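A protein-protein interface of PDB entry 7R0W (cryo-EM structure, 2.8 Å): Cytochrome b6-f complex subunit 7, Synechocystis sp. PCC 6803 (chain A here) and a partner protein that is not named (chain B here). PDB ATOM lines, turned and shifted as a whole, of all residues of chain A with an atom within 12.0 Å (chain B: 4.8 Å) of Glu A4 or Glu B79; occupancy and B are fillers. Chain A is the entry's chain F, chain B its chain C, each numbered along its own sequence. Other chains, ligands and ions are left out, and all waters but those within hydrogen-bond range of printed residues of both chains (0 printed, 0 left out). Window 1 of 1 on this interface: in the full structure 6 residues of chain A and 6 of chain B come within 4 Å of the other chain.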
ATOM      1  N   MET A   1      -5.581  -6.749 -28.542  1.00  0.00           N
ATOM      2  CA  MET A   1      -5.388  -5.329 -28.945  1.00  0.00           C
ATOM      3  C   MET A   1      -3.957  -4.950 -28.611  1.00  0.00           C
ATOM      4  O   MET A   1      -3.206  -5.780 -28.103  1.00  0.00           O
ATOM      5  CB  MET A   1      -6.388  -4.410 -28.242  1.00  0.00           C
ATOM      6  CG  MET A   1      -6.100  -4.149 -26.770  1.00  0.00           C
ATOM      7  SD  MET A   1      -7.258  -2.993 -26.003  1.00  0.00           S
ATOM      8  CE  MET A   1      -8.784  -3.375 -26.860  1.00  0.00           C
ATOM      9  N   THR A   2      -3.580  -3.701 -28.857  1.00  0.00           N
ATOM     10  CA  THR A   2      -2.208  -3.262 -28.669  1.00  0.00           C
ATOM     11  C   THR A   2      -2.080  -2.369 -27.443  1.00  0.00           C
ATOM     12  O   THR A   2      -3.054  -1.790 -26.955  1.00  0.00           O
ATOM     13  CB  THR A   2      -1.707  -2.502 -29.902  1.00  0.00           C
ATOM     14  OG1 THR A   2      -2.369  -1.236 -29.990  1.00  0.00           O
ATOM     15  CG2 THR A   2      -1.983  -3.295 -31.168  1.00  0.00           C
ATOM     16  N   ALA A   3      -0.842  -2.261 -26.955  1.00  0.00           N
ATOM     17  CA  ALA A   3      -0.577  -1.452 -25.771  1.00  0.00           C
ATOM     18  C   ALA A   3      -0.908   0.006 -26.040  1.00  0.00           C
ATOM     19  O   ALA A   3      -1.500   0.687 -25.195  1.00  0.00           O
ATOM     20  CB  ALA A   3       0.883  -1.603 -25.348  1.00  0.00           C
ATOM     21  N   GLU A   4      -0.535   0.501 -27.219  1.00  0.00           N
ATOM     22  CA  GLU A   4      -0.753   1.904 -27.540  1.00  0.00           C
ATOM     23  C   GLU A   4      -2.238   2.200 -27.697  1.00  0.00           C
ATOM     24  O   GLU A   4      -2.676   3.325 -27.433  1.00  0.00           O
ATOM     25  CB  GLU A   4       0.063   2.267 -28.791  1.00  0.00           C
ATOM     26  CG  GLU A   4      -0.264   1.505 -30.092  1.00  0.00           C
ATOM     27  CD  GLU A   4      -1.665   1.735 -30.637  1.00  0.00           C
ATOM     28  OE1 GLU A   4      -2.278   2.776 -30.322  1.00  0.00           O
ATOM     29  OE2 GLU A   4      -2.162   0.856 -31.371  1.00  0.00           O
ATOM     30  N   SER A   5      -3.024   1.210 -28.119  1.00  0.00           N
ATOM     31  CA  SER A   5      -4.451   1.423 -28.305  1.00  0.00           C
ATOM     32  C   SER A   5      -5.164   1.677 -26.986  1.00  0.00           C
ATOM     33  O   SER A   5      -6.241   2.276 -26.991  1.00  0.00           O
ATOM     34  CB  SER A   5      -5.083   0.217 -29.000  1.00  0.00           C
ATOM     35  OG  SER A   5      -5.400  -0.803 -28.069  1.00  0.00           O
ATOM     36  N   MET A   6      -4.562   1.282 -25.862  1.00  0.00           N
ATOM     37  CA  MET A   6      -5.188   1.327 -24.545  1.00  0.00           C
ATOM     38  C   MET A   6      -5.231   2.719 -23.927  1.00  0.00           C
ATOM     39  O   MET A   6      -5.742   2.858 -22.811  1.00  0.00           O
ATOM     40  CB  MET A   6      -4.466   0.382 -23.583  1.00  0.00           C
ATOM     41  CG  MET A   6      -4.823  -1.075 -23.786  1.00  0.00           C
ATOM     42  SD  MET A   6      -3.912  -2.180 -22.699  1.00  0.00           S
ATOM     43  CE  MET A   6      -4.386  -3.765 -23.378  1.00  0.00           C
ATOM     44  N   LEU A   7      -4.722   3.747 -24.602  1.00  0.00           N
ATOM     45  CA  LEU A   7      -4.856   5.103 -24.077  1.00  0.00           C
ATOM     46  C   LEU A   7      -6.284   5.624 -24.210  1.00  0.00           C
ATOM     47  O   LEU A   7      -6.908   6.009 -23.216  1.00  0.00           O
ATOM     48  CB  LEU A   7      -3.877   6.035 -24.793  1.00  0.00           C
ATOM     49  CG  LEU A   7      -3.428   7.254 -23.985  1.00  0.00           C
ATOM     50  CD1 LEU A   7      -2.036   7.687 -24.407  1.00  0.00           C
ATOM     51  CD2 LEU A   7      -4.412   8.400 -24.138  1.00  0.00           C
ATOM     52  N   ALA A   8      -6.825   5.641 -25.430  1.00  0.00           N
ATOM     53  CA  ALA A   8      -8.169   6.177 -25.631  1.00  0.00           C
ATOM     54  C   ALA A   8      -9.248   5.216 -25.146  1.00  0.00           C
ATOM     55  O   ALA A   8     -10.117   5.593 -24.346  1.00  0.00           O
ATOM     56  CB  ALA A   8      -8.378   6.505 -27.110  1.00  0.00           C
ATOM     57  N   ASN A   9      -9.204   3.965 -25.606  1.00  0.00           N
ATOM     58  CA  ASN A   9     -10.244   3.024 -25.217  1.00  0.00           C
ATOM     59  C   ASN A   9     -10.191   2.774 -23.722  1.00  0.00           C
ATOM     60  O   ASN A   9     -11.227   2.533 -23.105  1.00  0.00           O
ATOM     61  CB  ASN A   9     -10.105   1.707 -25.969  1.00  0.00           C
ATOM     62  CG  ASN A   9      -8.718   1.178 -25.912  1.00  0.00           C
ATOM     63  OD1 ASN A   9      -7.838   1.852 -25.397  1.00  0.00           O
ATOM     64  ND2 ASN A   9      -8.501  -0.025 -26.427  1.00  0.00           N
ATOM     65  N   GLY A  10      -8.997   2.782 -23.129  1.00  0.00           N
ATOM     66  CA  GLY A  10      -8.912   2.598 -21.692  1.00  0.00           C
ATOM     67  C   GLY A  10      -9.544   3.746 -20.933  1.00  0.00           C
ATOM     68  O   GLY A  10     -10.176   3.535 -19.895  1.00  0.00           O
ATOM     69  N   ALA A  11      -9.451   4.964 -21.472  1.00  0.00           N
ATOM     70  CA  ALA A  11     -10.088   6.104 -20.822  1.00  0.00           C
ATOM     71  C   ALA A  11     -11.601   6.002 -20.938  1.00  0.00           C
ATOM     72  O   ALA A  11     -12.334   6.286 -19.976  1.00  0.00           O
ATOM     73  CB  ALA A  11      -9.585   7.407 -21.438  1.00  0.00           C
ATOM     74  N   PHE A  12     -12.088   5.560 -22.098  1.00  0.00           N
ATOM     75  CA  PHE A  12     -13.528   5.405 -22.246  1.00  0.00           C
ATOM     76  C   PHE A  12     -14.031   4.245 -21.408  1.00  0.00           C
ATOM     77  O   PHE A  12     -15.131   4.315 -20.857  1.00  0.00           O
ATOM     78  CB  PHE A  12     -13.899   5.203 -23.714  1.00  0.00           C
ATOM     79  CG  PHE A  12     -13.315   6.233 -24.632  1.00  0.00           C
ATOM     80  CD1 PHE A  12     -13.232   7.558 -24.241  1.00  0.00           C
ATOM     81  CD2 PHE A  12     -12.848   5.880 -25.886  1.00  0.00           C
ATOM     82  CE1 PHE A  12     -12.694   8.510 -25.082  1.00  0.00           C
ATOM     83  CE2 PHE A  12     -12.314   6.828 -26.734  1.00  0.00           C
ATOM     84  CZ  PHE A  12     -12.239   8.146 -26.332  1.00  0.00           C
ATOM     85  N   ILE A  13     -13.235   3.184 -21.281  1.00  0.00           N
ATOM     86  CA  ILE A  13     -13.592   2.075 -20.407  1.00  0.00           C
ATOM     87  C   ILE A  13     -13.646   2.552 -18.965  1.00  0.00           C
ATOM     88  O   ILE A  13     -14.490   2.108 -18.183  1.00  0.00           O
ATOM     89  CB  ILE A  13     -12.598   0.914 -20.588  1.00  0.00           C
ATOM     90  CG1 ILE A  13     -12.926   0.138 -21.863  1.00  0.00           C
ATOM     91  CG2 ILE A  13     -12.630  -0.015 -19.385  1.00  0.00           C
ATOM     92  CD1 ILE A  13     -11.772  -0.673 -22.396  1.00  0.00           C
ATOM     93  N   GLU B  77       4.396   2.941 -37.602  1.00  0.00           N
ATOM     94  CA  GLU B  77       3.559   2.381 -36.548  1.00  0.00           C
ATOM     95  C   GLU B  77       3.765   0.878 -36.456  1.00  0.00           C
ATOM     96  O   GLU B  77       4.133   0.226 -37.434  1.00  0.00           O
ATOM     97  CB  GLU B  77       2.075   2.684 -36.782  1.00  0.00           C
ATOM     98  CG  GLU B  77       1.758   4.161 -36.901  1.00  0.00           C
ATOM     99  CD  GLU B  77       1.618   4.609 -38.341  1.00  0.00           C
ATOM    100  OE1 GLU B  77       2.444   4.187 -39.175  1.00  0.00           O
ATOM    101  OE2 GLU B  77       0.682   5.380 -38.638  1.00  0.00           O
ATOM    102  N   VAL B  78       3.497   0.332 -35.273  1.00  0.00           N
ATOM    103  CA  VAL B  78       3.533  -1.107 -35.028  1.00  0.00           C
ATOM    104  C   VAL B  78       2.273  -1.484 -34.266  1.00  0.00           C
ATOM    105  O   VAL B  78       2.007  -0.931 -33.192  1.00  0.00           O
ATOM    106  CB  VAL B  78       4.775  -1.540 -34.229  1.00  0.00           C
ATOM    107  CG1 VAL B  78       4.948  -3.048 -34.310  1.00  0.00           C
ATOM    108  CG2 VAL B  78       6.018  -0.849 -34.735  1.00  0.00           C
ATOM    109  N   GLU B  79       1.504  -2.420 -34.812  1.00  0.00           N
ATOM    110  CA  GLU B  79       0.314  -2.927 -34.136  1.00  0.00           C
ATOM    111  C   GLU B  79       0.657  -4.245 -33.443  1.00  0.00           C
ATOM    112  O   GLU B  79       0.267  -5.334 -33.866  1.00  0.00           O
ATOM    113  CB  GLU B  79      -0.829  -3.099 -35.131  1.00  0.00           C
ATOM    114  CG  GLU B  79      -1.215  -1.833 -35.883  1.00  0.00           C
ATOM    115  CD  GLU B  79      -1.298  -0.614 -34.987  1.00  0.00           C
ATOM    116  OE1 GLU B  79      -2.032  -0.665 -33.979  1.00  0.00           O
ATOM    117  OE2 GLU B  79      -0.630   0.396 -35.293  1.00  0.00           O
ATOM    118  N   ILE B  80       1.410  -4.125 -32.354  1.00  0.00           N
ATOM    119  CA  ILE B  80       1.822  -5.284 -31.567  1.00  0.00           C
ATOM    120  C   ILE B  80       0.843  -5.476 -30.415  1.00  0.00           C
ATOM    121  O   ILE B  80       0.408  -4.489 -29.806  1.00  0.00           O
ATOM    122  CB  ILE B  80       3.267  -5.130 -31.063  1.00  0.00           C
ATOM    123  CG1 ILE B  80       3.977  -6.485 -31.057  1.00  0.00           C
ATOM    124  CG2 ILE B  80       3.306  -4.499 -29.675  1.00  0.00           C
ATOM    125  CD1 ILE B  80       5.473  -6.383 -31.165  1.00  0.00           C
ATOM    126  N   PRO B  81       0.467  -6.710 -30.077  1.00  0.00           N
ATOM    127  CA  PRO B  81      -0.403  -6.914 -28.915  1.00  0.00           C
ATOM    128  C   PRO B  81       0.232  -6.400 -27.633  1.00  0.00           C
ATOM    129  O   PRO B  81       1.454  -6.407 -27.471  1.00  0.00           O
ATOM    130  CB  PRO B  81      -0.589  -8.435 -28.873  1.00  0.00           C
ATOM    131  CG  PRO B  81      -0.316  -8.885 -30.261  1.00  0.00           C
ATOM    132  CD  PRO B  81       0.766  -7.982 -30.755  1.00  0.00           C
ATOM    133  N   GLU B  91       1.107 -11.574 -34.506  1.00  0.00           N
ATOM    134  CA  GLU B  91       1.371 -10.718 -35.653  1.00  0.00           C
ATOM    135  C   GLU B  91       1.731  -9.314 -35.187  1.00  0.00           C
ATOM    136  O   GLU B  91       1.142  -8.794 -34.235  1.00  0.00           O
ATOM    137  CB  GLU B  91       0.161 -10.690 -36.602  1.00  0.00           C
ATOM    138  CG  GLU B  91      -0.825  -9.548 -36.385  1.00  0.00           C
ATOM    139  CD  GLU B  91      -1.411  -9.537 -34.986  1.00  0.00           C
ATOM    140  OE1 GLU B  91      -1.569 -10.629 -34.399  1.00  0.00           O
ATOM    141  OE2 GLU B  91      -1.708  -8.439 -34.471  1.00  0.00           O
ATOM    142  N   ALA B  92       2.717  -8.715 -35.852  1.00  0.00           N
ATOM    143  CA  ALA B  92       3.119  -7.330 -35.616  1.00  0.00           C
ATOM    144  C   ALA B  92       2.975  -6.569 -36.930  1.00  0.00           C
ATOM    145  O   ALA B  92       3.835  -6.663 -37.807  1.00  0.00           O
ATOM    146  CB  ALA B  92       4.546  -7.256 -35.081  1.00  0.00           C
ATOM    147  N   VAL B  93       1.854  -5.872 -37.097  1.00  0.00           N
ATOM    148  CA  VAL B  93       1.549  -5.188 -38.351  1.00  0.00           C
ATOM    149  C   VAL B  93       2.310  -3.865 -38.345  1.00  0.00           C
ATOM    150  O   VAL B  93       1.923  -2.921 -37.655  1.00  0.00           O
ATOM    151  CB  VAL B  93       0.047  -4.974 -38.535  1.00  0.00           C
ATOM    152  CG1 VAL B  93      -0.243  -4.445 -39.927  1.00  0.00           C
ATOM    153  CG2 VAL B  93      -0.705  -6.269 -38.278  1.00  0.00           C
ATOM    154  N   LYS B  95       2.943  -0.699 -39.867  1.00  0.00           N
ATOM    155  CA  LYS B  95       2.396   0.254 -40.822  1.00  0.00           C
ATOM    156  C   LYS B  95       3.467   1.260 -41.223  1.00  0.00           C
ATOM    157  O   LYS B  95       4.106   1.881 -40.364  1.00  0.00           O
ATOM    158  CB  LYS B  95       1.188   0.979 -40.230  1.00  0.00           C
ATOM    159  CG  LYS B  95       0.223   0.075 -39.484  1.00  0.00           C
ATOM    160  CD  LYS B  95      -1.215   0.374 -39.868  1.00  0.00           C
ATOM    161  CE  LYS B  95      -2.194  -0.380 -38.988  1.00  0.00           C
ATOM    162  NZ  LYS B  95      -2.002  -1.852 -39.075  1.00  0.00           N
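The side-chain carboxylate (OE1) of Glu B79 lies close to the side-chain carboxylate (OE2) of Glu A4 (3.0 Å).
O of Val B93 sits at hydrogen-bond distance from N of Glu B79. The side-chain sulfur of Met A1 lies within hydrogen-bond range of the side-chain hydroxyl of Ser A5, at 3.5 Å. ND2 of Asn A9 is in hydrogen-bond range of SD of Met A1, 3.2 Å away. The side-chain hydroxyl of Thr A2 lies within hydrogen-bond range of the side-chain carboxylate of Glu A4. O of Thr A2 is in hydrogen-bond range of OG of Ser A5, 2.8 Å away.
Met A1 touches Pro B81. Glu B79 touches Thr A2 (C to CG2, 3.6 Å). Thr A2 touches Ile B80 (CB to O, 2.9 Å). N of Ala A3 touches O of Ile B80, at 3.8 Å.
Printed residues of chain B within 4 Å of Met A1: Pro B81. Of the printed residues of chain B, Thr A2 touches Glu B79 (3.6 Å) and Ile B80 (2.9 Å). Printed residues of chain B within 4 Å of Ala A3: Ile B80 (3.8 Å). Ser A5 touches none of the printed residues of chain B. Phe A12 touches none of the printed residues of chain B. No residue of chain A comes within 4 Å of Glu B77. No residue of chain A comes within 4 Å of Val B78. Glu B79 touches just these residues of chain A: Thr A2 and Glu A4. Ile B80 touches just these residues of chain A: Thr A2 (2.9 Å) and Ala A3 (3.8 Å). Pro B81 touches just one residue of chain A: Met A1 (3.1 Å). No residue of chain A comes within 4 Å of Ala B92. No residue of chain A comes within 4 Å of Lys B95.
Of the 9 printed residues of chain B, 3 touch a printed residue of chain A. Hydrophobic or aromatic side chains of chain B within 4 Å of the printed part of chain A: Pro B81. Of the 13 printed residues of chain A, 4 touch a printed residue of chain B. Among the printed residues, no Asp or Glu carboxylate lies within 4 Å of a Lys or Arg side-chain nitrogen of the other chain.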
